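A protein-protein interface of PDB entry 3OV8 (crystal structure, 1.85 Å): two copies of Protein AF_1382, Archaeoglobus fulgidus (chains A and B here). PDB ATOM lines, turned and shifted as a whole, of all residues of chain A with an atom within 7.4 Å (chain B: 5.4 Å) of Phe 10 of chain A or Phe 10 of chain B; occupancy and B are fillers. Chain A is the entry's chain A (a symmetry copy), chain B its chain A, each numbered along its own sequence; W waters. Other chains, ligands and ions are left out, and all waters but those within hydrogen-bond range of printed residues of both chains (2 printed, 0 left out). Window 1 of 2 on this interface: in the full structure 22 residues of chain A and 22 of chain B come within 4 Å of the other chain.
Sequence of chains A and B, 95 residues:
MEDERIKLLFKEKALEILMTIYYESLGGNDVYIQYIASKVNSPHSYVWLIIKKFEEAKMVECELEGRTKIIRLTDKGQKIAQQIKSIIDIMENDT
NZ of Lys 11 of chain B sits at hydrogen-bond distance from O of Lys 7 of chain A (2.8 Å). O of Leu 9 of chain B is in hydrogen-bond range of N of Lys 11 of chain A (2.8 Å). The backbone carbonyl oxygen (O) of Leu 9 of chain A sits at hydrogen-bond distance from the backbone NH (N) of Lys 11 of chain B (2.8 Å). The backbone carbonyl oxygen (O) of Lys 7 of chain B is in hydrogen-bond range of the side-chain amino group (NZ) of Lys 11 of chain A, 2.8 Å away. The backbone carbonyl oxygen of Phe 10 of chain B sits at hydrogen-bond distance from the side-chain amino group of Lys 11 of chain A (3.0 Å). NZ of Lys 11 of chain B is in hydrogen-bond range of O of Phe 10 of chain A, 3.0 Å away.
Among the printed residues, merely in contact across the chains: Leu 8 of chain A with Lys 11 of chain B (3.7 Å), Leu 9 of chain A with Phe 10 of chain B (3.3 Å), Phe 10 of chain A with Leu 9 of chain B (3.3 Å), Phe 10 of chain A with Phe 10 of chain B (3.2 Å), Lys 11 of chain A with Leu 8 of chain B (3.7 Å), Lys 11 of chain A with Lys 11 of chain B (3.8 Å), Ala 14 of chain A with Leu 8 of chain B (3.3 Å), Ile 80 of chain A with Leu 9 of chain B (3.9 Å), Gln 83 of chain A with Ile 87 of chain B (3.6 Å), Ile 84 of chain A with Ile 87 of chain B (3.7 Å), Ile 87 of chain A with Ile 84 of chain B (3.7 Å) and Ile 87 of chain A with Ile 87 of chain B (3.7 Å).
Phe 10 of chain A touches three residues of chain B. Of the printed residues of chain A, Phe 10 of chain B touches Leu 9 (3.3 Å), Phe 10 (3.2 Å) and Lys 11 (3.0 Å). Of the printed residues of chain B, Ile 84 of chain A touches Ile 87. Of the printed residues of chain B, Ile 87 of chain A touches Ile 84 and Ile 87. Of the printed residues of chain B, Gln 83 of chain A touches Ile 87 (3.6 Å). Printed residues of chain B within 4 Å of Lys 7 of chain A: Lys 11. Printed residues of chain B within 4 Å of Lys 11 of chain A: Lys 7, Leu 8, Leu 9, Phe 10 and Lys 11. The nearest printed residue of chain A that does not touch Leu 8 of chain B is Leu 15 of chain A (5.6 Å).
Of the 10 printed residues of chain B, 7 touch a printed residue of chain A. Printed residues of chain B that touch a printed residue of chain A: Lys 7, Leu 8, Leu 9, Phe 10, Lys 11, Ile 84 and Ile 87. Hydrophobic or aromatic side chains of chain B that line the printed part of chain A: Leu 9, Phe 10, Ile 84 and Ile 87. Among the printed residues, no Asp or Glu carboxylate lies within 4 Å of a Lys or Arg side-chain nitrogen of the other chain.
Leu 9 of chain A touches Lys 11 of chain B, and with the chains exchanged Lys 11 of chain A touches Leu 9 of chain B. Phe 10 of chain B touches its own counterpart, Phe 10 of chain A. Phe 10 of chain A touches Lys 11 of chain B, and with the chains exchanged Lys 11 of chain A touches Phe 10 of chain B. Ile 87 of chain B touches its own counterpart, Ile 87 of chain A. 10 positions are printed for both chains. Of the 18 pairs that touch across the chains among the printed residues, 15 have their exchanged pair printed and touching as well.
Water W1 bridges NZ of Lys 11 of chain B (2.9 Å) and O of Lys 7 of chain A (3.1 Å). Water W2 bridges NZ of Lys 11 of chain A and O of Lys 7 of chain B.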
ATOM      1  N   GLU A   4     -21.179   8.743  18.587  1.00  0.00           N
ATOM      2  CA  GLU A   4     -21.270   8.293  19.972  1.00  0.00           C
ATOM      3  C   GLU A   4     -21.726   9.413  20.914  1.00  0.00           C
ATOM      4  O   GLU A   4     -22.633   9.225  21.730  1.00  0.00           O
ATOM      5  CB  GLU A   4     -19.940   7.706  20.431  1.00  0.00           C
ATOM      6  CG  GLU A   4     -19.933   6.189  20.456  1.00  0.00           C
ATOM      7  CD  GLU A   4     -20.942   5.625  21.444  1.00  0.00           C
ATOM      8  OE1 GLU A   4     -21.208   6.291  22.467  1.00  0.00           O
ATOM      9  OE2 GLU A   4     -21.471   4.519  21.196  1.00  0.00           O
ATOM     10  N   ARG A   5     -21.085  10.573  20.811  1.00  0.00           N
ATOM     11  CA  ARG A   5     -21.624  11.767  21.434  1.00  0.00           C
ATOM     12  C   ARG A   5     -22.902  12.076  20.678  1.00  0.00           C
ATOM     13  O   ARG A   5     -23.843  12.654  21.221  1.00  0.00           O
ATOM     14  CB  ARG A   5     -20.648  12.934  21.323  1.00  0.00           C
ATOM     15  CG  ARG A   5     -19.362  12.756  22.105  1.00  0.00           C
ATOM     16  CD  ARG A   5     -18.326  13.773  21.664  1.00  0.00           C
ATOM     17  NE  ARG A   5     -17.194  13.836  22.585  1.00  0.00           N
ATOM     18  CZ  ARG A   5     -16.238  14.757  22.527  1.00  0.00           C
ATOM     19  NH1 ARG A   5     -16.278  15.693  21.586  1.00  0.00           N
ATOM     20  NH2 ARG A   5     -15.245  14.746  23.407  1.00  0.00           N
ATOM     21  N   ILE A   6     -22.920  11.671  19.413  1.00  0.00           N
ATOM     22  CA  ILE A   6     -24.110  11.786  18.584  1.00  0.00           C
ATOM     23  C   ILE A   6     -25.240  10.932  19.141  1.00  0.00           C
ATOM     24  O   ILE A   6     -26.375  11.394  19.252  1.00  0.00           O
ATOM     25  CB  ILE A   6     -23.820  11.374  17.129  1.00  0.00           C
ATOM     26  CG1 ILE A   6     -22.864  12.377  16.485  1.00  0.00           C
ATOM     27  CG2 ILE A   6     -25.105  11.309  16.335  1.00  0.00           C
ATOM     28  CD1 ILE A   6     -23.334  13.814  16.617  1.00  0.00           C
ATOM     29  N   LYS A   7     -24.926   9.694  19.506  1.00  0.00           N
ATOM     30  CA  LYS A   7     -25.925   8.805  20.096  1.00  0.00           C
ATOM     31  C   LYS A   7     -26.478   9.389  21.397  1.00  0.00           C
ATOM     32  O   LYS A   7     -27.602   9.102  21.785  1.00  0.00           O
ATOM     33  CB  LYS A   7     -25.346   7.413  20.358  1.00  0.00           C
ATOM     34  CG  LYS A   7     -25.010   6.638  19.091  1.00  0.00           C
ATOM     35  CD  LYS A   7     -24.905   5.147  19.374  1.00  0.00           C
ATOM     36  CE  LYS A   7     -26.226   4.594  19.894  1.00  0.00           C
ATOM     37  NZ  LYS A   7     -26.259   3.103  19.866  1.00  0.00           N
ATOM     38  N   LEU A   8     -25.684  10.217  22.062  1.00  0.00           N
ATOM     39  CA  LEU A   8     -26.124  10.836  23.311  1.00  0.00           C
ATOM     40  C   LEU A   8     -27.391  11.674  23.090  1.00  0.00           C
ATOM     41  O   LEU A   8     -28.325  11.630  23.887  1.00  0.00           O
ATOM     42  CB  LEU A   8     -24.983  11.681  23.888  1.00  0.00           C
ATOM     43  CG  LEU A   8     -25.174  12.524  25.148  1.00  0.00           C
ATOM     44  CD1 LEU A   8     -25.787  11.720  26.279  1.00  0.00           C
ATOM     45  CD2 LEU A   8     -23.829  13.092  25.568  1.00  0.00           C
ATOM     46  N   LEU A   9     -27.437  12.409  21.982  1.00  0.00           N
ATOM     47  CA  LEU A   9     -28.566  13.291  21.720  1.00  0.00           C
ATOM     48  C   LEU A   9     -29.542  12.786  20.653  1.00  0.00           C
ATOM     49  O   LEU A   9     -30.727  13.121  20.686  1.00  0.00           O
ATOM     50  CB  LEU A   9     -28.068  14.679  21.326  1.00  0.00           C
ATOM     51  CG  LEU A   9     -27.606  15.545  22.495  1.00  0.00           C
ATOM     52  CD1 LEU A   9     -26.926  16.799  21.989  1.00  0.00           C
ATOM     53  CD2 LEU A   9     -28.784  15.875  23.407  1.00  0.00           C
ATOM     54  N   PHE A  10     -29.043  12.004  19.701  1.00  0.00           N
ATOM     55  CA  PHE A  10     -29.844  11.619  18.540  1.00  0.00           C
ATOM     56  C   PHE A  10     -30.207  10.134  18.457  1.00  0.00           C
ATOM     57  O   PHE A  10     -29.488   9.268  18.961  1.00  0.00           O
ATOM     58  CB  PHE A  10     -29.098  11.985  17.256  1.00  0.00           C
ATOM     59  CG  PHE A  10     -28.950  13.466  17.039  1.00  0.00           C
ATOM     60  CD1 PHE A  10     -29.977  14.201  16.475  1.00  0.00           C
ATOM     61  CD2 PHE A  10     -27.780  14.114  17.391  1.00  0.00           C
ATOM     62  CE1 PHE A  10     -29.841  15.565  16.269  1.00  0.00           C
ATOM     63  CE2 PHE A  10     -27.637  15.474  17.188  1.00  0.00           C
ATOM     64  CZ  PHE A  10     -28.670  16.199  16.629  1.00  0.00           C
ATOM     65  N   LYS A  11     -31.326   9.864  17.798  1.00  0.00           N
ATOM     66  CA  LYS A  11     -31.647   8.531  17.317  1.00  0.00           C
ATOM     67  C   LYS A  11     -30.771   8.263  16.092  1.00  0.00           C
ATOM     68  O   LYS A  11     -31.026   8.782  15.002  1.00  0.00           O
ATOM     69  CB  LYS A  11     -33.139   8.432  16.983  1.00  0.00           C
ATOM     70  CG  LYS A  11     -34.081   8.713  18.201  1.00  0.00           C
ATOM     71  CD  LYS A  11     -34.177   7.528  19.161  1.00  0.00           C
ATOM     72  CE  LYS A  11     -34.831   7.917  20.503  1.00  0.00           C
ATOM     73  NZ  LYS A  11     -36.197   8.490  20.342  1.00  0.00           N
ATOM     74  N   GLU A  12     -29.733   7.453  16.297  1.00  0.00           N
ATOM     75  CA  GLU A  12     -28.658   7.245  15.329  1.00  0.00           C
ATOM     76  C   GLU A  12     -29.158   6.762  13.968  1.00  0.00           C
ATOM     77  O   GLU A  12     -28.700   7.236  12.929  1.00  0.00           O
ATOM     78  CB  GLU A  12     -27.640   6.252  15.895  1.00  0.00           C
ATOM     79  CG  GLU A  12     -26.748   5.589  14.862  1.00  0.00           C
ATOM     80  CD  GLU A  12     -25.524   6.420  14.523  1.00  0.00           C
ATOM     81  OE1 GLU A  12     -25.166   7.306  15.328  1.00  0.00           O
ATOM     82  OE2 GLU A  12     -24.919   6.186  13.451  1.00  0.00           O
ATOM     83  N   LYS A  13     -30.098   5.823  13.976  1.00  0.00           N
ATOM     84  CA  LYS A  13     -30.587   5.247  12.725  1.00  0.00           C
ATOM     85  C   LYS A  13     -31.381   6.265  11.921  1.00  0.00           C
ATOM     86  O   LYS A  13     -31.160   6.425  10.718  1.00  0.00           O
ATOM     87  CB  LYS A  13     -31.404   3.978  12.984  1.00  0.00           C
ATOM     88  CG  LYS A  13     -30.554   2.804  13.462  1.00  0.00           C
ATOM     89  CD  LYS A  13     -29.359   2.587  12.533  1.00  0.00           C
ATOM     90  CE  LYS A  13     -28.487   1.417  12.977  1.00  0.00           C
ATOM     91  NZ  LYS A  13     -27.787   1.681  14.264  1.00  0.00           N
ATOM     92  N   ALA A  14     -32.290   6.974  12.579  1.00  0.00           N
ATOM     93  CA  ALA A  14     -33.096   7.990  11.897  1.00  0.00           C
ATOM     94  C   ALA A  14     -32.222   9.137  11.406  1.00  0.00           C
ATOM     95  O   ALA A  14     -32.428   9.679  10.304  1.00  0.00           O
ATOM     96  CB  ALA A  14     -34.204   8.521  12.817  1.00  0.00           C
ATOM     97  N   LEU A  15     -31.241   9.503  12.220  1.00  0.00           N
ATOM     98  CA  LEU A  15     -30.312  10.575  11.856  1.00  0.00           C
ATOM     99  C   LEU A  15     -29.558  10.226  10.578  1.00  0.00           C
ATOM    100  O   LEU A  15     -29.443  11.047   9.666  1.00  0.00           O
ATOM    101  CB  LEU A  15     -29.285  10.810  12.963  1.00  0.00           C
ATOM    102  CG  LEU A  15     -28.133  11.735  12.554  1.00  0.00           C
ATOM    103  CD1 LEU A  15     -28.654  13.131  12.326  1.00  0.00           C
ATOM    104  CD2 LEU A  15     -27.036  11.735  13.621  1.00  0.00           C
ATOM    105  N   GLU A  16     -29.009   9.022  10.523  1.00  0.00           N
ATOM    106  CA  GLU A  16     -28.200   8.674   9.363  1.00  0.00           C
ATOM    107  C   GLU A  16     -29.058   8.571   8.093  1.00  0.00           C
ATOM    108  O   GLU A  16     -28.590   8.882   7.005  1.00  0.00           O
ATOM    109  CB  GLU A  16     -27.331   7.437   9.598  1.00  0.00           C
ATOM    110  CG  GLU A  16     -28.059   6.129   9.769  1.00  0.00           C
ATOM    111  CD  GLU A  16     -27.117   4.987  10.153  1.00  0.00           C
ATOM    112  OE1 GLU A  16     -25.984   5.275  10.600  1.00  0.00           O
ATOM    113  OE2 GLU A  16     -27.510   3.807  10.011  1.00  0.00           O
ATOM    114  N   ILE A  80     -33.978  21.338   8.696  1.00  0.00           N
ATOM    115  CA  ILE A  80     -33.620  20.503   9.829  1.00  0.00           C
ATOM    116  C   ILE A  80     -32.281  19.799   9.584  1.00  0.00           C
ATOM    117  O   ILE A  80     -31.394  19.835  10.432  1.00  0.00           O
ATOM    118  CB  ILE A  80     -34.733  19.492  10.139  1.00  0.00           C
ATOM    119  CG1 ILE A  80     -35.942  20.239  10.727  1.00  0.00           C
ATOM    120  CG2 ILE A  80     -34.235  18.421  11.114  1.00  0.00           C
ATOM    121  CD1 ILE A  80     -37.210  19.431  10.748  1.00  0.00           C
ATOM    122  N   GLN A  83     -29.368  22.129   9.968  1.00  0.00           N
ATOM    123  CA  GLN A  83     -29.077  22.481  11.353  1.00  0.00           C
ATOM    124  C   GLN A  83     -28.374  21.320  12.060  1.00  0.00           C
ATOM    125  O   GLN A  83     -27.451  21.523  12.849  1.00  0.00           O
ATOM    126  CB  GLN A  83     -30.361  22.848  12.099  1.00  0.00           C
ATOM    127  CG  GLN A  83     -31.014  24.120  11.605  1.00  0.00           C
ATOM    128  CD  GLN A  83     -30.239  25.361  12.008  1.00  0.00           C
ATOM    129  OE1 GLN A  83     -29.952  25.576  13.191  1.00  0.00           O
ATOM    130  NE2 GLN A  83     -29.888  26.178  11.026  1.00  0.00           N
ATOM    131  N   ILE A  84     -28.805  20.098  11.766  1.00  0.00           N
ATOM    132  CA  ILE A  84     -28.158  18.922  12.326  1.00  0.00           C
ATOM    133  C   ILE A  84     -26.701  18.816  11.851  1.00  0.00           C
ATOM    134  O   ILE A  84     -25.793  18.491  12.629  1.00  0.00           O
ATOM    135  CB  ILE A  84     -28.946  17.647  11.989  1.00  0.00           C
ATOM    136  CG1 ILE A  84     -30.247  17.614  12.800  1.00  0.00           C
ATOM    137  CG2 ILE A  84     -28.102  16.408  12.293  1.00  0.00           C
ATOM    138  CD1 ILE A  84     -31.198  16.502  12.386  1.00  0.00           C
ATOM    139  N   LYS A  85     -26.478  19.105  10.576  1.00  0.00           N
ATOM    140  CA  LYS A  85     -25.122  19.169  10.037  1.00  0.00           C
ATOM    141  C   LYS A  85     -24.229  20.073  10.896  1.00  0.00           C
ATOM    142  O   LYS A  85     -23.108  19.704  11.255  1.00  0.00           O
ATOM    143  CB  LYS A  85     -25.156  19.657   8.589  1.00  0.00           C
ATOM    144  CG  LYS A  85     -23.781  19.943   7.984  1.00  0.00           C
ATOM    145  CD  LYS A  85     -23.907  20.539   6.586  1.00  0.00           C
ATOM    146  CE  LYS A  85     -22.542  20.878   6.014  1.00  0.00           C
ATOM    147  NZ  LYS A  85     -21.726  19.646   5.835  1.00  0.00           N
ATOM    148  N   ILE A  87     -24.690  20.936  14.084  1.00  0.00           N
ATOM    149  CA  ILE A  87     -24.522  20.292  15.390  1.00  0.00           C
ATOM    150  C   ILE A  87     -23.443  19.213  15.313  1.00  0.00           C
ATOM    151  O   ILE A  87     -22.547  19.145  16.149  1.00  0.00           O
ATOM    152  CB  ILE A  87     -25.838  19.665  15.885  1.00  0.00           C
ATOM    153  CG1 ILE A  87     -26.858  20.771  16.198  1.00  0.00           C
ATOM    154  CG2 ILE A  87     -25.595  18.824  17.138  1.00  0.00           C
ATOM    155  CD1 ILE A  87     -28.250  20.265  16.485  1.00  0.00           C
ATOM    156  N   ILE A  88     -23.519  18.371  14.290  1.00  0.00           N
ATOM    157  CA  ILE A  88     -22.518  17.331  14.116  1.00  0.00           C
ATOM    158  C   ILE A  88     -21.119  17.937  14.035  1.00  0.00           C
ATOM    159  O   ILE A  88     -20.200  17.470  14.717  1.00  0.00           O
ATOM    160  CB  ILE A  88     -22.807  16.463  12.868  1.00  0.00           C
ATOM    161  CG1 ILE A  88     -24.103  15.673  13.064  1.00  0.00           C
ATOM    162  CG2 ILE A  88     -21.650  15.515  12.592  1.00  0.00           C
ATOM    163  CD1 ILE A  88     -24.580  14.965  11.792  1.00  0.00           C
ATOM    164  N   MET A  91     -20.113  19.179  17.493  1.00  0.00           N
ATOM    165  CA  MET A  91     -19.833  18.063  18.393  1.00  0.00           C
ATOM    166  C   MET A  91     -18.451  17.467  18.152  1.00  0.00           C
ATOM    167  O   MET A  91     -17.760  17.080  19.095  1.00  0.00           O
ATOM    168  CB  MET A  91     -20.891  16.971  18.250  1.00  0.00           C
ATOM    169  CG  MET A  91     -20.826  15.925  19.347  1.00  0.00           C
ATOM    170  SD  MET A  91     -21.423  16.565  20.927  1.00  0.00           S
ATOM    171  CE  MET A  91     -23.183  16.503  20.649  1.00  0.00           C
ATOM    172  N   ILE B   6     -40.191  15.028  17.588  1.00  0.00           N
ATOM    173  CA  ILE B   6     -38.936  15.189  18.304  1.00  0.00           C
ATOM    174  C   ILE B   6     -38.330  13.835  18.644  1.00  0.00           C
ATOM    175  O   ILE B   6     -37.137  13.616  18.434  1.00  0.00           O
ATOM    176  CB  ILE B   6     -39.130  16.006  19.596  1.00  0.00           C
ATOM    177  CG1 ILE B   6     -39.506  17.446  19.249  1.00  0.00           C
ATOM    178  CG2 ILE B   6     -37.864  15.993  20.422  1.00  0.00           C
ATOM    179  CD1 ILE B   6     -38.542  18.092  18.272  1.00  0.00           C
ATOM    180  N   LYS B   7     -39.154  12.924  19.149  1.00  0.00           N
ATOM    181  CA  LYS B   7     -38.685  11.576  19.467  1.00  0.00           C
ATOM    182  C   LYS B   7     -38.161  10.869  18.216  1.00  0.00           C
ATOM    183  O   LYS B   7     -37.313   9.992  18.301  1.00  0.00           O
ATOM    184  CB  LYS B   7     -39.793  10.738  20.109  1.00  0.00           C
ATOM    185  CG  LYS B   7     -40.200  11.217  21.497  1.00  0.00           C
ATOM    186  CD  LYS B   7     -40.919  10.117  22.265  1.00  0.00           C
ATOM    187  CE  LYS B   7     -40.016   8.905  22.460  1.00  0.00           C
ATOM    188  NZ  LYS B   7     -40.562   7.960  23.477  1.00  0.00           N
ATOM    189  N   LEU B   8     -38.665  11.265  17.055  1.00  0.00           N
ATOM    190  CA  LEU B   8     -38.222  10.659  15.801  1.00  0.00           C
ATOM    191  C   LEU B   8     -36.711  10.849  15.605  1.00  0.00           C
ATOM    192  O   LEU B   8     -36.006   9.928  15.199  1.00  0.00           O
ATOM    193  CB  LEU B   8     -39.021  11.258  14.638  1.00  0.00           C
ATOM    194  CG  LEU B   8     -38.717  10.885  13.187  1.00  0.00           C
ATOM    195  CD1 LEU B   8     -38.652   9.382  12.992  1.00  0.00           C
ATOM    196  CD2 LEU B   8     -39.784  11.491  12.291  1.00  0.00           C
ATOM    197  N   LEU B   9     -36.209  12.036  15.933  1.00  0.00           N
ATOM    198  CA  LEU B   9     -34.800  12.334  15.717  1.00  0.00           C
ATOM    199  C   LEU B   9     -33.943  12.342  16.985  1.00  0.00           C
ATOM    200  O   LEU B   9     -32.742  12.073  16.925  1.00  0.00           O
ATOM    201  CB  LEU B   9     -34.651  13.676  15.003  1.00  0.00           C
ATOM    202  CG  LEU B   9     -34.918  13.632  13.501  1.00  0.00           C
ATOM    203  CD1 LEU B   9     -34.968  15.032  12.931  1.00  0.00           C
ATOM    204  CD2 LEU B   9     -33.864  12.778  12.801  1.00  0.00           C
ATOM    205  N   PHE B  10     -34.549  12.670  18.122  1.00  0.00           N
ATOM    206  CA  PHE B  10     -33.789  12.884  19.351  1.00  0.00           C
ATOM    207  C   PHE B  10     -34.024  11.850  20.456  1.00  0.00           C
ATOM    208  O   PHE B  10     -35.092  11.242  20.550  1.00  0.00           O
ATOM    209  CB  PHE B  10     -34.121  14.261  19.928  1.00  0.00           C
ATOM    210  CG  PHE B  10     -33.646  15.407  19.080  1.00  0.00           C
ATOM    211  CD1 PHE B  10     -32.339  15.852  19.165  1.00  0.00           C
ATOM    212  CD2 PHE B  10     -34.512  16.042  18.207  1.00  0.00           C
ATOM    213  CE1 PHE B  10     -31.900  16.913  18.388  1.00  0.00           C
ATOM    214  CE2 PHE B  10     -34.081  17.101  17.430  1.00  0.00           C
ATOM    215  CZ  PHE B  10     -32.773  17.533  17.519  1.00  0.00           C
ATOM    216  N   LYS B  11     -33.008  11.681  21.294  1.00  0.00           N
ATOM    217  CA  LYS B  11     -33.159  11.025  22.581  1.00  0.00           C
ATOM    218  C   LYS B  11     -33.866  12.008  23.517  1.00  0.00           C
ATOM    219  O   LYS B  11     -33.261  12.964  24.007  1.00  0.00           O
ATOM    220  CB  LYS B  11     -31.790  10.604  23.126  1.00  0.00           C
ATOM    221  CG  LYS B  11     -31.018   9.608  22.198  1.00  0.00           C
ATOM    222  CD  LYS B  11     -31.542   8.176  22.300  1.00  0.00           C
ATOM    223  CE  LYS B  11     -31.009   7.279  21.164  1.00  0.00           C
ATOM    224  NZ  LYS B  11     -29.521   7.221  21.116  1.00  0.00           N
ATOM    225  N   GLU B  12     -35.155  11.759  23.741  1.00  0.00           N
ATOM    226  CA  GLU B  12     -36.058  12.687  24.417  1.00  0.00           C
ATOM    227  C   GLU B  12     -35.578  13.089  25.811  1.00  0.00           C
ATOM    228  O   GLU B  12     -35.646  14.259  26.183  1.00  0.00           O
ATOM    229  CB  GLU B  12     -37.458  12.072  24.503  1.00  0.00           C
ATOM    230  CG  GLU B  12     -38.363  12.682  25.557  1.00  0.00           C
ATOM    231  CD  GLU B  12     -39.097  13.914  25.060  1.00  0.00           C
ATOM    232  OE1 GLU B  12     -39.205  14.083  23.826  1.00  0.00           O
ATOM    233  OE2 GLU B  12     -39.569  14.711  25.903  1.00  0.00           O
ATOM    234  N   LEU B  15     -32.346  15.190  25.594  1.00  0.00           N
ATOM    235  CA  LEU B  15     -32.716  16.477  25.002  1.00  0.00           C
ATOM    236  C   LEU B  15     -33.335  17.397  26.048  1.00  0.00           C
ATOM    237  O   LEU B  15     -32.976  18.572  26.151  1.00  0.00           O
ATOM    238  CB  LEU B  15     -33.732  16.291  23.875  1.00  0.00           C
ATOM    239  CG  LEU B  15     -34.353  17.601  23.377  1.00  0.00           C
ATOM    240  CD1 LEU B  15     -33.302  18.441  22.699  1.00  0.00           C
ATOM    241  CD2 LEU B  15     -35.518  17.317  22.425  1.00  0.00           C
ATOM    242  N   ILE B  84     -30.369  23.201  18.502  1.00  0.00           N
ATOM    243  CA  ILE B  84     -31.502  22.330  18.772  1.00  0.00           C
ATOM    244  C   ILE B  84     -32.791  23.144  18.960  1.00  0.00           C
ATOM    245  O   ILE B  84     -33.864  22.772  18.464  1.00  0.00           O
ATOM    246  CB  ILE B  84     -31.229  21.433  19.989  1.00  0.00           C
ATOM    247  CG1 ILE B  84     -30.188  20.369  19.624  1.00  0.00           C
ATOM    248  CG2 ILE B  84     -32.524  20.769  20.458  1.00  0.00           C
ATOM    249  CD1 ILE B  84     -29.691  19.564  20.816  1.00  0.00           C
ATOM    250  N   ILE B  87     -34.144  23.795  15.603  1.00  0.00           N
ATOM    251  CA  ILE B  87     -34.753  22.582  15.050  1.00  0.00           C
ATOM    252  C   ILE B  87     -36.140  22.363  15.654  1.00  0.00           C
ATOM    253  O   ILE B  87     -37.112  22.112  14.947  1.00  0.00           O
ATOM    254  CB  ILE B  87     -33.880  21.341  15.313  1.00  0.00           C
ATOM    255  CG1 ILE B  87     -32.574  21.442  14.510  1.00  0.00           C
ATOM    256  CG2 ILE B  87     -34.625  20.066  14.918  1.00  0.00           C
ATOM    257  CD1 ILE B  87     -31.552  20.388  14.856  1.00  0.00           C
HETATM  258  O   HOH W   1     -28.485   6.890  23.787  1.00  0.00           O
HETATM  259  O   HOH W   2     -37.687   6.906  18.447  1.00  0.00           O
